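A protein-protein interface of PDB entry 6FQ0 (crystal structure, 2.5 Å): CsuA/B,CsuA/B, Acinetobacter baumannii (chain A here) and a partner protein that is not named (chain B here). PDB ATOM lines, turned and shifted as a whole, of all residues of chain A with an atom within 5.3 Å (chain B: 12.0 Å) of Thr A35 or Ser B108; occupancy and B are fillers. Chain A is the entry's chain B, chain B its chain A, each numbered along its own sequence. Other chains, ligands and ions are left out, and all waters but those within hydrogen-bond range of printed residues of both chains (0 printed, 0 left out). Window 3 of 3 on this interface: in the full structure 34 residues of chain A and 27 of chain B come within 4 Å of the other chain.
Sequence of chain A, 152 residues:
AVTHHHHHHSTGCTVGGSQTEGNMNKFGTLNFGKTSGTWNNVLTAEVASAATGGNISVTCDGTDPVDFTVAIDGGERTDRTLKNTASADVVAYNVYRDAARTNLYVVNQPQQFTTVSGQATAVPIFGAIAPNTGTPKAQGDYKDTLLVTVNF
Hydrophobic or aromatic side chains of chain A within 4 Å of the printed part of chain B: Leu A30, Phe A32, Leu A82 and Tyr A142. Along chain A the printed residues that touch a printed residue of chain B span positions 30 to 142. Printed residues of chain B that touch a printed residue of chain A: Ser B108, Lys B109, Val B110 and Phe B112. Among the printed residues, no Asp or Glu carboxylate lies within 4 Å of a Lys or Arg side-chain nitrogen of the other chain.
The side-chain amide oxygen (OD1) of Asn A31 sits close to the backbone carbonyl oxygen (O) of Ser B108 (3.3 Å). The backbone NH (N) of Phe A32 lies within hydrogen-bond range of the backbone carbonyl oxygen (O) of Ser B108, at 3.1 Å. The backbone carbonyl oxygen of Gly A33 is in hydrogen-bond range of the backbone NH of Ser B108, 3.2 Å away. N of Lys B109 is in hydrogen-bond range of O of Tyr A142. N of Leu A30 lies within hydrogen-bond range of O of Val B110, at 2.9 Å.
Of the printed residues of chain B, Leu A30 touches Ser B108, Lys B109, Val B110 and Phe B112. Asn A31 touches just these residues of chain B: Ser B108 (3.3 Å) and Lys B109 (3.4 Å). Gly A33 touches just one residue of chain B: Ser B108. No residue of chain B comes within 4 Å of Lys A34. Of chain B, only Ser B108 comes within 4 Å of Thr A35. No residue of chain B comes within 4 Å of Ser A36. Of chain B, only Ser B108 (3.6 Å), Lys B109 (3.4 Å) and Val B110 (3.8 Å) come within 4 Å of Leu A82. No residue of chain B comes within 4 Å of Lys A137. Of chain A, only Leu A30 (3.9 Å), Asn A31 (3.3 Å), Phe A32 (3.1 Å), Gly A33 (3.2 Å), Thr A35 (3.4 Å), Leu A82 (3.6 Å) and Tyr A142 (3.2 Å) come within 4 Å of Ser B108. Of the printed residues of chain A, Val B110 touches Leu A30 (2.9 Å), Phe A32 (3.6 Å) and Leu A82 (3.8 Å). Of the printed residues of chain A, Phe B112 touches Leu A30 (3.8 Å). The nearest residue of chain B that does not touch Thr A35 is Lys B109 (6.7 Å).
N of Gly A33 lies within hydrogen-bond range of OD1 of Asn A31, at 2.9 Å. The backbone NH (N) of Leu A82 sits at hydrogen-bond distance from the backbone carbonyl oxygen (O) of Val A91 (3.1 Å).
Ser B108 touches Leu A30 (O to O, 3.9 Å). Leu A30 touches Lys B109. Leu A30 touches Phe B112. CG of Asn A31 touches CG of Lys B109 (3.4 Å). CG1 of Val B110 touches CE2 of Phe A32, at 3.6 Å. Thr A35 touches Ser B108 (CG2 to OG, 3.4 Å). OG of Ser B108 touches CD1 of Leu A82, 3.6 Å away. Leu A82 touches Lys B109. Val B110 touches Leu A82 (N to CD2, 3.8 Å). Ser B108 touches Tyr A142 (CA to O, 3.2 Å).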
ATOM      1  N   LEU A  30      11.424  20.705  -1.791  1.00  0.00           N
ATOM      2  CA  LEU A  30      10.543  19.881  -2.612  1.00  0.00           C
ATOM      3  C   LEU A  30      11.393  19.176  -3.661  1.00  0.00           C
ATOM      4  O   LEU A  30      11.829  19.786  -4.639  1.00  0.00           O
ATOM      5  CB  LEU A  30       9.455  20.733  -3.252  1.00  0.00           C
ATOM      6  CG  LEU A  30       8.473  21.440  -2.321  1.00  0.00           C
ATOM      7  CD1 LEU A  30       7.727  22.523  -3.078  1.00  0.00           C
ATOM      8  CD2 LEU A  30       7.482  20.466  -1.708  1.00  0.00           C
ATOM      9  N   ASN A  31      11.648  17.887  -3.459  1.00  0.00           N
ATOM     10  CA  ASN A  31      12.376  17.081  -4.433  1.00  0.00           C
ATOM     11  C   ASN A  31      11.361  16.297  -5.259  1.00  0.00           C
ATOM     12  O   ASN A  31      10.776  15.321  -4.779  1.00  0.00           O
ATOM     13  CB  ASN A  31      13.369  16.145  -3.745  1.00  0.00           C
ATOM     14  CG  ASN A  31      14.364  15.527  -4.718  1.00  0.00           C
ATOM     15  OD1 ASN A  31      14.068  15.325  -5.897  1.00  0.00           O
ATOM     16  ND2 ASN A  31      15.562  15.240  -4.224  1.00  0.00           N
ATOM     17  N   PHE A  32      11.160  16.723  -6.502  1.00  0.00           N
ATOM     18  CA  PHE A  32      10.207  16.073  -7.388  1.00  0.00           C
ATOM     19  C   PHE A  32      10.778  14.829  -8.055  1.00  0.00           C
ATOM     20  O   PHE A  32      10.052  14.151  -8.793  1.00  0.00           O
ATOM     21  CB  PHE A  32       9.736  17.058  -8.457  1.00  0.00           C
ATOM     22  CG  PHE A  32       8.831  18.138  -7.934  1.00  0.00           C
ATOM     23  CD1 PHE A  32       7.469  17.918  -7.807  1.00  0.00           C
ATOM     24  CD2 PHE A  32       9.340  19.374  -7.577  1.00  0.00           C
ATOM     25  CE1 PHE A  32       6.635  18.912  -7.333  1.00  0.00           C
ATOM     26  CE2 PHE A  32       8.512  20.371  -7.103  1.00  0.00           C
ATOM     27  CZ  PHE A  32       7.158  20.141  -6.981  1.00  0.00           C
ATOM     28  N   GLY A  33      12.046  14.518  -7.821  1.00  0.00           N
ATOM     29  CA  GLY A  33      12.686  13.403  -8.486  1.00  0.00           C
ATOM     30  C   GLY A  33      13.337  13.851  -9.780  1.00  0.00           C
ATOM     31  O   GLY A  33      13.693  15.017  -9.967  1.00  0.00           O
ATOM     32  N   LYS A  34      13.495  12.897 -10.692  1.00  0.00           N
ATOM     33  CA  LYS A  34      13.994  13.218 -12.020  1.00  0.00           C
ATOM     34  C   LYS A  34      12.861  13.815 -12.846  1.00  0.00           C
ATOM     35  O   LYS A  34      11.785  13.221 -12.962  1.00  0.00           O
ATOM     36  CB  LYS A  34      14.567  11.975 -12.699  1.00  0.00           C
ATOM     37  CG  LYS A  34      15.442  12.285 -13.905  1.00  0.00           C
ATOM     38  CD  LYS A  34      16.032  11.020 -14.504  1.00  0.00           C
ATOM     39  CE  LYS A  34      16.872  11.327 -15.732  1.00  0.00           C
ATOM     40  NZ  LYS A  34      17.512  10.103 -16.287  1.00  0.00           N
ATOM     41  N   THR A  35      13.107  14.991 -13.426  1.00  0.00           N
ATOM     42  CA  THR A  35      12.096  15.697 -14.205  1.00  0.00           C
ATOM     43  C   THR A  35      12.526  15.880 -15.656  1.00  0.00           C
ATOM     44  O   THR A  35      11.973  16.723 -16.372  1.00  0.00           O
ATOM     45  CB  THR A  35      11.766  17.046 -13.558  1.00  0.00           C
ATOM     46  OG1 THR A  35      10.501  17.517 -14.042  1.00  0.00           O
ATOM     47  CG2 THR A  35      12.842  18.079 -13.854  1.00  0.00           C
ATOM     48  N   SER A  36      13.485  15.083 -16.111  1.00  0.00           N
ATOM     49  CA  SER A  36      14.003  15.174 -17.465  1.00  0.00           C
ATOM     50  C   SER A  36      13.281  14.150 -18.327  1.00  0.00           C
ATOM     51  O   SER A  36      12.961  13.051 -17.865  1.00  0.00           O
ATOM     52  CB  SER A  36      15.513  14.931 -17.498  1.00  0.00           C
ATOM     53  OG  SER A  36      16.061  15.258 -18.763  1.00  0.00           O
ATOM     54  N   GLY A  37      13.011  14.521 -19.567  1.00  0.00           N
ATOM     55  CA  GLY A  37      12.317  13.637 -20.488  1.00  0.00           C
ATOM     56  C   GLY A  37      10.826  13.907 -20.482  1.00  0.00           C
ATOM     57  O   GLY A  37      10.398  15.054 -20.605  1.00  0.00           O
ATOM     58  N   TRP A  39       6.811  12.418 -18.696  1.00  0.00           N
ATOM     59  CA  TRP A  39       6.115  11.669 -17.660  1.00  0.00           C
ATOM     60  C   TRP A  39       4.619  11.854 -17.875  1.00  0.00           C
ATOM     61  O   TRP A  39       4.170  12.917 -18.310  1.00  0.00           O
ATOM     62  CB  TRP A  39       6.520  12.123 -16.252  1.00  0.00           C
ATOM     63  CG  TRP A  39       6.353  13.594 -16.016  1.00  0.00           C
ATOM     64  CD1 TRP A  39       5.279  14.215 -15.448  1.00  0.00           C
ATOM     65  CD2 TRP A  39       7.285  14.630 -16.348  1.00  0.00           C
ATOM     66  NE1 TRP A  39       5.485  15.572 -15.403  1.00  0.00           N
ATOM     67  CE2 TRP A  39       6.709  15.853 -15.950  1.00  0.00           C
ATOM     68  CE3 TRP A  39       8.550  14.642 -16.943  1.00  0.00           C
ATOM     69  CZ2 TRP A  39       7.355  17.075 -16.128  1.00  0.00           C
ATOM     70  CZ3 TRP A  39       9.188  15.855 -17.118  1.00  0.00           C
ATOM     71  CH2 TRP A  39       8.591  17.055 -16.711  1.00  0.00           C
ATOM     72  N   LEU A  43       3.704  14.728 -10.937  1.00  0.00           N
ATOM     73  CA  LEU A  43       4.857  14.656 -10.049  1.00  0.00           C
ATOM     74  C   LEU A  43       4.532  15.373  -8.747  1.00  0.00           C
ATOM     75  O   LEU A  43       4.003  16.488  -8.762  1.00  0.00           O
ATOM     76  CB  LEU A  43       6.080  15.287 -10.712  1.00  0.00           C
ATOM     77  CG  LEU A  43       7.018  14.400 -11.533  1.00  0.00           C
ATOM     78  CD1 LEU A  43       6.261  13.316 -12.285  1.00  0.00           C
ATOM     79  CD2 LEU A  43       7.819  15.259 -12.498  1.00  0.00           C
ATOM     80  N   LEU A  82      11.175  25.471 -12.565  1.00  0.00           N
ATOM     81  CA  LEU A  82      12.532  25.029 -12.270  1.00  0.00           C
ATOM     82  C   LEU A  82      13.399  25.112 -13.520  1.00  0.00           C
ATOM     83  O   LEU A  82      12.965  24.748 -14.615  1.00  0.00           O
ATOM     84  CB  LEU A  82      12.525  23.594 -11.741  1.00  0.00           C
ATOM     85  CG  LEU A  82      11.685  23.305 -10.498  1.00  0.00           C
ATOM     86  CD1 LEU A  82      10.740  22.137 -10.751  1.00  0.00           C
ATOM     87  CD2 LEU A  82      12.579  23.024  -9.301  1.00  0.00           C
ATOM     88  N   VAL A  91      10.260  23.904 -16.187  1.00  0.00           N
ATOM     89  CA  VAL A  91       9.150  23.004 -15.897  1.00  0.00           C
ATOM     90  C   VAL A  91       8.282  23.648 -14.824  1.00  0.00           C
ATOM     91  O   VAL A  91       8.745  23.919 -13.710  1.00  0.00           O
ATOM     92  CB  VAL A  91       9.649  21.612 -15.466  1.00  0.00           C
ATOM     93  CG1 VAL A  91      10.853  21.734 -14.544  1.00  0.00           C
ATOM     94  CG2 VAL A  91       8.531  20.833 -14.790  1.00  0.00           C
ATOM     95  N   ILE A 129       3.655  18.944 -10.171  1.00  0.00           N
ATOM     96  CA  ILE A 129       4.021  19.232 -11.552  1.00  0.00           C
ATOM     97  C   ILE A 129       3.046  18.494 -12.461  1.00  0.00           C
ATOM     98  O   ILE A 129       2.853  17.282 -12.316  1.00  0.00           O
ATOM     99  CB  ILE A 129       5.476  18.827 -11.863  1.00  0.00           C
ATOM    100  CG1 ILE A 129       6.455  19.747 -11.128  1.00  0.00           C
ATOM    101  CG2 ILE A 129       5.735  18.864 -13.359  1.00  0.00           C
ATOM    102  CD1 ILE A 129       7.888  19.257 -11.154  1.00  0.00           C
ATOM    103  N   LYS A 137      11.841  16.955 -22.000  1.00  0.00           N
ATOM    104  CA  LYS A 137      12.778  17.949 -21.485  1.00  0.00           C
ATOM    105  C   LYS A 137      14.221  17.555 -21.784  1.00  0.00           C
ATOM    106  O   LYS A 137      14.941  17.087 -20.903  1.00  0.00           O
ATOM    107  CB  LYS A 137      12.586  18.136 -19.980  1.00  0.00           C
ATOM    108  CG  LYS A 137      11.234  18.714 -19.595  1.00  0.00           C
ATOM    109  CD  LYS A 137      11.058  20.121 -20.144  1.00  0.00           C
ATOM    110  CE  LYS A 137       9.590  20.511 -20.206  1.00  0.00           C
ATOM    111  NZ  LYS A 137       9.414  21.916 -20.663  1.00  0.00           N
ATOM    112  N   ASP A 141      19.828  18.411 -13.564  1.00  0.00           N
ATOM    113  CA  ASP A 141      19.352  19.152 -12.401  1.00  0.00           C
ATOM    114  C   ASP A 141      18.367  20.243 -12.794  1.00  0.00           C
ATOM    115  O   ASP A 141      18.507  20.868 -13.840  1.00  0.00           O
ATOM    116  CB  ASP A 141      20.526  19.782 -11.646  1.00  0.00           C
ATOM    117  CG  ASP A 141      21.491  18.753 -11.094  1.00  0.00           C
ATOM    118  OD1 ASP A 141      21.050  17.625 -10.789  1.00  0.00           O
ATOM    119  OD2 ASP A 141      22.692  19.074 -10.966  1.00  0.00           O
ATOM    120  N   TYR A 142      17.362  20.461 -11.949  1.00  0.00           N
ATOM    121  CA  TYR A 142      16.415  21.554 -12.115  1.00  0.00           C
ATOM    122  C   TYR A 142      16.220  22.199 -10.753  1.00  0.00           C
ATOM    123  O   TYR A 142      15.951  21.501  -9.772  1.00  0.00           O
ATOM    124  CB  TYR A 142      15.070  21.078 -12.681  1.00  0.00           C
ATOM    125  CG  TYR A 142      15.069  20.783 -14.169  1.00  0.00           C
ATOM    126  CD1 TYR A 142      15.741  19.683 -14.685  1.00  0.00           C
ATOM    127  CD2 TYR A 142      14.399  21.616 -15.057  1.00  0.00           C
ATOM    128  CE1 TYR A 142      15.731  19.413 -16.043  1.00  0.00           C
ATOM    129  CE2 TYR A 142      14.392  21.359 -16.417  1.00  0.00           C
ATOM    130  CZ  TYR A 142      15.061  20.256 -16.905  1.00  0.00           C
ATOM    131  OH  TYR A 142      15.053  19.997 -18.258  1.00  0.00           O
ATOM    132  N   SER B 108      15.858  17.292  -9.509  1.00  0.00           N
ATOM    133  CA  SER B 108      14.996  18.465  -9.596  1.00  0.00           C
ATOM    134  C   SER B 108      14.446  18.846  -8.227  1.00  0.00           C
ATOM    135  O   SER B 108      13.669  18.100  -7.629  1.00  0.00           O
ATOM    136  CB  SER B 108      13.846  18.211 -10.568  1.00  0.00           C
ATOM    137  OG  SER B 108      13.016  19.353 -10.690  1.00  0.00           O
ATOM    138  N   LYS B 109      14.848  20.014  -7.733  1.00  0.00           N
ATOM    139  CA  LYS B 109      14.543  20.419  -6.370  1.00  0.00           C
ATOM    140  C   LYS B 109      14.280  21.916  -6.318  1.00  0.00           C
ATOM    141  O   LYS B 109      15.014  22.704  -6.921  1.00  0.00           O
ATOM    142  CB  LYS B 109      15.692  20.065  -5.418  1.00  0.00           C
ATOM    143  CG  LYS B 109      15.871  18.575  -5.182  1.00  0.00           C
ATOM    144  CD  LYS B 109      17.337  18.178  -5.239  1.00  0.00           C
ATOM    145  CE  LYS B 109      18.158  18.917  -4.200  1.00  0.00           C
ATOM    146  NZ  LYS B 109      19.616  18.668  -4.374  1.00  0.00           N
ATOM    147  N   VAL B 110      13.237  22.300  -5.590  1.00  0.00           N
ATOM    148  CA  VAL B 110      12.965  23.697  -5.273  1.00  0.00           C
ATOM    149  C   VAL B 110      13.148  23.872  -3.771  1.00  0.00           C
ATOM    150  O   VAL B 110      12.535  23.150  -2.973  1.00  0.00           O
ATOM    151  CB  VAL B 110      11.564  24.130  -5.736  1.00  0.00           C
ATOM    152  CG1 VAL B 110      10.610  22.952  -5.735  1.00  0.00           C
ATOM    153  CG2 VAL B 110      11.028  25.259  -4.865  1.00  0.00           C
ATOM    154  N   SER B 111      14.004  24.814  -3.389  1.00  0.00           N
ATOM    155  CA  SER B 111      14.336  25.067  -1.995  1.00  0.00           C
ATOM    156  C   SER B 111      13.569  26.274  -1.469  1.00  0.00           C
ATOM    157  O   SER B 111      13.035  27.086  -2.230  1.00  0.00           O
ATOM    158  CB  SER B 111      15.842  25.291  -1.833  1.00  0.00           C
ATOM    159  OG  SER B 111      16.331  26.168  -2.831  1.00  0.00           O
ATOM    160  N   PHE B 112      13.522  26.384  -0.144  1.00  0.00           N
ATOM    161  CA  PHE B 112      12.806  27.453   0.535  1.00  0.00           C
ATOM    162  C   PHE B 112      13.788  28.453   1.131  1.00  0.00           C
ATOM    163  O   PHE B 112      14.833  28.070   1.665  1.00  0.00           O
ATOM    164  CB  PHE B 112      11.910  26.899   1.645  1.00  0.00           C
ATOM    165  CG  PHE B 112      10.869  25.937   1.159  1.00  0.00           C
ATOM    166  CD1 PHE B 112      10.325  26.064  -0.107  1.00  0.00           C
ATOM    167  CD2 PHE B 112      10.435  24.902   1.969  1.00  0.00           C
ATOM    168  CE1 PHE B 112       9.367  25.177  -0.556  1.00  0.00           C
ATOM    169  CE2 PHE B 112       9.478  24.012   1.526  1.00  0.00           C
ATOM    170  CZ  PHE B 112       8.945  24.149   0.261  1.00  0.00           C
